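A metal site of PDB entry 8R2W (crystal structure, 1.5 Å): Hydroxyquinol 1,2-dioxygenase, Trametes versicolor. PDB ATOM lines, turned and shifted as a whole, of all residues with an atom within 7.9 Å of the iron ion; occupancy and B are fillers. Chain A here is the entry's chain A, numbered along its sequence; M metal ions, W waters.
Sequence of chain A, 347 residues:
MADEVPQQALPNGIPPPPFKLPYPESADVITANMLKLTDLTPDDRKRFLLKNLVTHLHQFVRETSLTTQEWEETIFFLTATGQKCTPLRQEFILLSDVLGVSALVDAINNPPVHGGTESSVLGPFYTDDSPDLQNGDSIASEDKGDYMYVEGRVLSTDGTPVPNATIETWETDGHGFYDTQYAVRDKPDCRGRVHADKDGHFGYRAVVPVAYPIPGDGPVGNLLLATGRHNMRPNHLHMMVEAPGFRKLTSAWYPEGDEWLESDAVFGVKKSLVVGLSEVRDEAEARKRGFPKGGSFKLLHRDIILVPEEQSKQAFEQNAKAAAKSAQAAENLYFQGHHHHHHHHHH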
ATOM      1  N   VAL A 121       8.613 -20.885  18.658  1.00  0.00           N
ATOM      2  CA  VAL A 121       8.130 -19.673  19.293  1.00  0.00           C
ATOM      3  C   VAL A 121       6.821 -19.210  18.664  1.00  0.00           C
ATOM      4  O   VAL A 121       6.536 -19.326  17.449  1.00  0.00           O
ATOM      5  CB  VAL A 121       9.155 -18.541  19.244  1.00  0.00           C
ATOM      6  CG1 VAL A 121      10.478 -18.946  19.904  1.00  0.00           C
ATOM      7  CG2 VAL A 121       9.362 -18.031  17.836  1.00  0.00           C
ATOM      8  N   LEU A 122       6.025 -18.606  19.544  1.00  0.00           N
ATOM      9  CA  LEU A 122       4.709 -18.082  19.198  1.00  0.00           C
ATOM     10  C   LEU A 122       4.845 -16.866  18.292  1.00  0.00           C
ATOM     11  O   LEU A 122       4.110 -16.705  17.322  1.00  0.00           O
ATOM     12  CB  LEU A 122       3.985 -17.712  20.498  1.00  0.00           C
ATOM     13  CG  LEU A 122       2.566 -17.166  20.329  1.00  0.00           C
ATOM     14  CD1 LEU A 122       1.620 -18.270  19.928  1.00  0.00           C
ATOM     15  CD2 LEU A 122       2.082 -16.481  21.608  1.00  0.00           C
ATOM     16  N   GLY A 123       5.697 -15.933  18.701  1.00  0.00           N
ATOM     17  CA  GLY A 123       5.815 -14.651  18.047  1.00  0.00           C
ATOM     18  C   GLY A 123       4.695 -13.692  18.420  1.00  0.00           C
ATOM     19  O   GLY A 123       3.870 -14.021  19.244  1.00  0.00           O
ATOM     20  N   PRO A 124       4.748 -12.459  17.874  1.00  0.00           N
ATOM     21  CA  PRO A 124       3.885 -11.363  18.299  1.00  0.00           C
ATOM     22  C   PRO A 124       2.527 -11.215  17.644  1.00  0.00           C
ATOM     23  O   PRO A 124       1.820 -10.261  17.935  1.00  0.00           O
ATOM     24  CB  PRO A 124       4.721 -10.132  17.883  1.00  0.00           C
ATOM     25  CG  PRO A 124       5.456 -10.606  16.622  1.00  0.00           C
ATOM     26  CD  PRO A 124       5.785 -12.040  16.927  1.00  0.00           C
ATOM     27  N   PHE A 125       2.186 -12.106  16.689  1.00  0.00           N
ATOM     28  CA  PHE A 125       1.047 -11.833  15.823  1.00  0.00           C
ATOM     29  C   PHE A 125      -0.079 -12.858  15.952  1.00  0.00           C
ATOM     30  O   PHE A 125      -0.966 -12.894  15.045  1.00  0.00           O
ATOM     31  CB  PHE A 125       1.521 -11.684  14.363  1.00  0.00           C
ATOM     32  CG  PHE A 125       2.113 -10.334  14.062  1.00  0.00           C
ATOM     33  CD1 PHE A 125       1.386  -9.171  14.275  1.00  0.00           C
ATOM     34  CD2 PHE A 125       3.411 -10.229  13.553  1.00  0.00           C
ATOM     35  CE1 PHE A 125       1.937  -7.916  14.031  1.00  0.00           C
ATOM     36  CE2 PHE A 125       3.963  -8.974  13.309  1.00  0.00           C
ATOM     37  CZ  PHE A 125       3.217  -7.827  13.504  1.00  0.00           C
ATOM     38  N   TYR A 126      -0.077 -13.640  17.038  1.00  0.00           N
ATOM     39  CA  TYR A 126      -1.166 -14.542  17.379  1.00  0.00           C
ATOM     40  C   TYR A 126      -2.372 -13.734  17.859  1.00  0.00           C
ATOM     41  O   TYR A 126      -2.226 -12.796  18.618  1.00  0.00           O
ATOM     42  CB  TYR A 126      -0.749 -15.563  18.446  1.00  0.00           C
ATOM     43  CG  TYR A 126      -1.919 -16.361  18.950  1.00  0.00           C
ATOM     44  CD1 TYR A 126      -2.516 -17.311  18.142  1.00  0.00           C
ATOM     45  CD2 TYR A 126      -2.571 -16.009  20.112  1.00  0.00           C
ATOM     46  CE1 TYR A 126      -3.669 -17.972  18.551  1.00  0.00           C
ATOM     47  CE2 TYR A 126      -3.725 -16.656  20.539  1.00  0.00           C
ATOM     48  CZ  TYR A 126      -4.279 -17.640  19.749  1.00  0.00           C
ATOM     49  OH  TYR A 126      -5.443 -18.282  20.154  1.00  0.00           O
ATOM     50  N   TRP A 170      -1.558 -19.328  11.361  1.00  0.00           N
ATOM     51  CA  TRP A 170      -1.461 -17.940  10.910  1.00  0.00           C
ATOM     52  C   TRP A 170      -0.131 -17.748  10.193  1.00  0.00           C
ATOM     53  O   TRP A 170       0.816 -18.499  10.440  1.00  0.00           O
ATOM     54  CB  TRP A 170      -1.738 -16.905  12.039  1.00  0.00           C
ATOM     55  CG  TRP A 170      -0.724 -16.836  13.167  1.00  0.00           C
ATOM     56  CD1 TRP A 170       0.195 -15.861  13.377  1.00  0.00           C
ATOM     57  CD2 TRP A 170      -0.599 -17.747  14.268  1.00  0.00           C
ATOM     58  NE1 TRP A 170       0.951 -16.137  14.490  1.00  0.00           N
ATOM     59  CE2 TRP A 170       0.477 -17.273  15.070  1.00  0.00           C
ATOM     60  CE3 TRP A 170      -1.237 -18.942  14.662  1.00  0.00           C
ATOM     61  CZ2 TRP A 170       0.894 -17.988  16.193  1.00  0.00           C
ATOM     62  CZ3 TRP A 170      -0.811 -19.642  15.752  1.00  0.00           C
ATOM     63  CH2 TRP A 170       0.242 -19.142  16.538  1.00  0.00           C
ATOM     64  N   GLU A 171      -0.094 -16.754   9.294  1.00  0.00           N
ATOM     65  CA  GLU A 171       1.044 -16.532   8.445  1.00  0.00           C
ATOM     66  C   GLU A 171       0.977 -15.107   7.893  1.00  0.00           C
ATOM     67  O   GLU A 171      -0.097 -14.505   7.792  1.00  0.00           O
ATOM     68  CB  GLU A 171       1.083 -17.499   7.258  1.00  0.00           C
ATOM     69  CG  GLU A 171      -0.167 -17.533   6.394  1.00  0.00           C
ATOM     70  CD  GLU A 171      -0.110 -18.369   5.132  1.00  0.00           C
ATOM     71  OE1 GLU A 171       1.019 -18.701   4.668  1.00  0.00           O
ATOM     72  OE2 GLU A 171      -1.220 -18.609   4.572  1.00  0.00           O
ATOM     73  N   THR A 172       2.142 -14.669   7.433  1.00  0.00           N
ATOM     74  CA  THR A 172       2.249 -13.571   6.507  1.00  0.00           C
ATOM     75  C   THR A 172       1.453 -13.906   5.259  1.00  0.00           C
ATOM     76  O   THR A 172       1.326 -15.064   4.854  1.00  0.00           O
ATOM     77  CB  THR A 172       3.747 -13.261   6.290  1.00  0.00           C
ATOM     78  OG1 THR A 172       3.717 -12.004   5.637  1.00  0.00           O
ATOM     79  CG2 THR A 172       4.397 -14.325   5.428  1.00  0.00           C
ATOM     80  N   TYR A 178       1.566  -9.520   7.817  1.00  0.00           N
ATOM     81  CA  TYR A 178       0.447 -10.026   8.606  1.00  0.00           C
ATOM     82  C   TYR A 178      -0.741  -9.069   8.500  1.00  0.00           C
ATOM     83  O   TYR A 178      -0.585  -7.884   8.250  1.00  0.00           O
ATOM     84  CB  TYR A 178       0.837 -10.275  10.061  1.00  0.00           C
ATOM     85  CG  TYR A 178       1.719 -11.486  10.287  1.00  0.00           C
ATOM     86  CD1 TYR A 178       1.155 -12.725  10.569  1.00  0.00           C
ATOM     87  CD2 TYR A 178       3.097 -11.405  10.221  1.00  0.00           C
ATOM     88  CE1 TYR A 178       1.950 -13.866  10.720  1.00  0.00           C
ATOM     89  CE2 TYR A 178       3.909 -12.516  10.418  1.00  0.00           C
ATOM     90  CZ  TYR A 178       3.335 -13.752  10.668  1.00  0.00           C
ATOM     91  OH  TYR A 178       4.121 -14.905  10.811  1.00  0.00           O
ATOM     92  N   TYR A 212      10.132 -12.999   6.065  1.00  0.00           N
ATOM     93  CA  TYR A 212       9.295 -12.069   6.795  1.00  0.00           C
ATOM     94  C   TYR A 212      10.187 -11.049   7.495  1.00  0.00           C
ATOM     95  O   TYR A 212      10.920 -11.389   8.435  1.00  0.00           O
ATOM     96  CB  TYR A 212       8.355 -12.771   7.765  1.00  0.00           C
ATOM     97  CG  TYR A 212       7.540 -11.761   8.531  1.00  0.00           C
ATOM     98  CD1 TYR A 212       6.638 -10.940   7.856  1.00  0.00           C
ATOM     99  CD2 TYR A 212       7.782 -11.518   9.854  1.00  0.00           C
ATOM    100  CE1 TYR A 212       5.973  -9.922   8.533  1.00  0.00           C
ATOM    101  CE2 TYR A 212       7.139 -10.514  10.555  1.00  0.00           C
ATOM    102  CZ  TYR A 212       6.210  -9.725   9.885  1.00  0.00           C
ATOM    103  OH  TYR A 212       5.506  -8.719  10.512  1.00  0.00           O
ATOM    104  N   ARG A 233      12.976 -13.031   9.425  1.00  0.00           N
ATOM    105  CA  ARG A 233      12.668 -14.417   9.718  1.00  0.00           C
ATOM    106  C   ARG A 233      12.515 -15.162   8.395  1.00  0.00           C
ATOM    107  O   ARG A 233      12.035 -14.631   7.416  1.00  0.00           O
ATOM    108  CB  ARG A 233      11.325 -14.580  10.440  1.00  0.00           C
ATOM    109  CG  ARG A 233      11.200 -13.876  11.794  1.00  0.00           C
ATOM    110  CD  ARG A 233      10.214 -14.611  12.657  1.00  0.00           C
ATOM    111  NE  ARG A 233      10.665 -15.951  12.968  1.00  0.00           N
ATOM    112  CZ  ARG A 233       9.956 -16.940  13.466  1.00  0.00           C
ATOM    113  NH1 ARG A 233       8.656 -16.814  13.730  1.00  0.00           N
ATOM    114  NH2 ARG A 233      10.588 -18.071  13.703  1.00  0.00           N
ATOM    115  N   PRO A 234      12.882 -16.450   8.360  1.00  0.00           N
ATOM    116  CA  PRO A 234      12.605 -17.261   7.189  1.00  0.00           C
ATOM    117  C   PRO A 234      11.101 -17.397   7.079  1.00  0.00           C
ATOM    118  O   PRO A 234      10.360 -17.261   8.055  1.00  0.00           O
ATOM    119  CB  PRO A 234      13.257 -18.601   7.504  1.00  0.00           C
ATOM    120  CG  PRO A 234      13.218 -18.676   9.021  1.00  0.00           C
ATOM    121  CD  PRO A 234      13.428 -17.247   9.470  1.00  0.00           C
ATOM    122  N   ASN A 235      10.682 -17.791   5.861  1.00  0.00           N
ATOM    123  CA  ASN A 235       9.314 -18.175   5.605  1.00  0.00           C
ATOM    124  C   ASN A 235       8.805 -19.180   6.639  1.00  0.00           C
ATOM    125  O   ASN A 235       9.498 -20.115   7.024  1.00  0.00           O
ATOM    126  CB  ASN A 235       9.147 -18.669   4.156  1.00  0.00           C
ATOM    127  CG  ASN A 235       9.969 -19.860   3.676  1.00  0.00           C
ATOM    128  OD1 ASN A 235      10.068 -20.102   2.461  1.00  0.00           O
ATOM    129  ND2 ASN A 235      10.609 -20.583   4.582  1.00  0.00           N
ATOM    130  N   HIS A 236       7.569 -18.987   7.126  1.00  0.00           N
ATOM    131  CA  HIS A 236       7.032 -19.908   8.133  1.00  0.00           C
ATOM    132  C   HIS A 236       5.514 -19.805   8.214  1.00  0.00           C
ATOM    133  O   HIS A 236       4.912 -18.775   7.915  1.00  0.00           O
ATOM    134  CB  HIS A 236       7.666 -19.666   9.516  1.00  0.00           C
ATOM    135  CG  HIS A 236       7.390 -18.310  10.049  1.00  0.00           C
ATOM    136  ND1 HIS A 236       8.025 -17.177   9.595  1.00  0.00           N
ATOM    137  CD2 HIS A 236       6.495 -17.920  10.986  1.00  0.00           C
ATOM    138  CE1 HIS A 236       7.518 -16.127  10.250  1.00  0.00           C
ATOM    139  NE2 HIS A 236       6.592 -16.556  11.079  1.00  0.00           N
ATOM    140  N   LEU A 237       4.926 -20.899   8.693  1.00  0.00           N
ATOM    141  CA  LEU A 237       3.493 -21.049   8.912  1.00  0.00           C
ATOM    142  C   LEU A 237       3.327 -21.471  10.387  1.00  0.00           C
ATOM    143  O   LEU A 237       3.801 -22.528  10.780  1.00  0.00           O
ATOM    144  CB  LEU A 237       2.907 -22.112   7.983  1.00  0.00           C
ATOM    145  CG  LEU A 237       1.432 -22.444   8.235  1.00  0.00           C
ATOM    146  CD1 LEU A 237       0.516 -21.284   7.915  1.00  0.00           C
ATOM    147  CD2 LEU A 237       1.015 -23.696   7.465  1.00  0.00           C
ATOM    148  N   HIS A 238       2.680 -20.639  11.210  1.00  0.00           N
ATOM    149  CA  HIS A 238       2.439 -21.002  12.601  1.00  0.00           C
ATOM    150  C   HIS A 238       1.400 -22.099  12.735  1.00  0.00           C
ATOM    151  O   HIS A 238       0.399 -22.108  11.983  1.00  0.00           O
ATOM    152  CB  HIS A 238       1.975 -19.789  13.399  1.00  0.00           C
ATOM    153  CG  HIS A 238       2.971 -18.669  13.413  1.00  0.00           C
ATOM    154  ND1 HIS A 238       3.873 -18.586  14.454  1.00  0.00           N
ATOM    155  CD2 HIS A 238       3.233 -17.617  12.599  1.00  0.00           C
ATOM    156  CE1 HIS A 238       4.675 -17.534  14.252  1.00  0.00           C
ATOM    157  NE2 HIS A 238       4.315 -16.883  13.141  1.00  0.00           N
ATOM    158  N   ALA A 252       5.687 -24.191  14.442  1.00  0.00           N
ATOM    159  CA  ALA A 252       5.643 -23.578  13.122  1.00  0.00           C
ATOM    160  C   ALA A 252       6.377 -24.477  12.161  1.00  0.00           C
ATOM    161  O   ALA A 252       7.264 -25.237  12.561  1.00  0.00           O
ATOM    162  CB  ALA A 252       6.231 -22.197  13.100  1.00  0.00           C
ATOM    163  N   TYR A 254       8.653 -24.487   8.584  1.00  0.00           N
ATOM    164  CA  TYR A 254       9.584 -23.601   7.906  1.00  0.00           C
ATOM    165  C   TYR A 254       9.966 -24.159   6.541  1.00  0.00           C
ATOM    166  O   TYR A 254      10.723 -25.114   6.444  1.00  0.00           O
ATOM    167  CB  TYR A 254      10.851 -23.438   8.748  1.00  0.00           C
ATOM    168  CG  TYR A 254      10.629 -22.765  10.096  1.00  0.00           C
ATOM    169  CD1 TYR A 254      10.625 -21.394  10.226  1.00  0.00           C
ATOM    170  CD2 TYR A 254      10.340 -23.551  11.206  1.00  0.00           C
ATOM    171  CE1 TYR A 254      10.361 -20.799  11.454  1.00  0.00           C
ATOM    172  CE2 TYR A 254      10.058 -22.979  12.429  1.00  0.00           C
ATOM    173  CZ  TYR A 254      10.094 -21.606  12.549  1.00  0.00           C
ATOM    174  OH  TYR A 254       9.789 -20.996  13.764  1.00  0.00           O
ATOM    175  N   VAL A 266      14.731 -14.481  15.515  1.00  0.00           N
ATOM    176  CA  VAL A 266      14.115 -14.809  16.791  1.00  0.00           C
ATOM    177  C   VAL A 266      14.385 -16.249  17.208  1.00  0.00           C
ATOM    178  O   VAL A 266      13.717 -16.753  18.107  1.00  0.00           O
ATOM    179  CB  VAL A 266      12.618 -14.498  16.774  1.00  0.00           C
ATOM    180  CG1 VAL A 266      12.386 -13.043  16.477  1.00  0.00           C
ATOM    181  CG2 VAL A 266      11.858 -15.422  15.805  1.00  0.00           C
HETATM  182 FE    FE M   1       5.231 -15.423  12.147  1.00  0.00          FE
HETATM  183  O   HOH W   1       6.210 -13.988  13.618  1.00  0.00           O
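O of Trp 170 sits at hydrogen-bond distance from N of His 238, at 2.9 Å. The backbone carbonyl oxygen (O) of Leu 122 sits close to a ring nitrogen (ND1) of His 238. The guanidinium group (NH1) of Arg 233 sits close to a ring nitrogen (NE2) of His 236 (3.4 Å). A ring nitrogen (ND1) of His 236 sits at hydrogen-bond distance from the backbone carbonyl oxygen (O) of Pro 234 (2.8 Å).
Within 4 Å of the iron ion: Tyr 178, His 236 and His 238.
The iron ion is bound by the side-chain hydroxyl (OH) of Tyr 178, a ring nitrogen (NE2) of His 238, a ring nitrogen (NE2) of His 236 and water W1.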
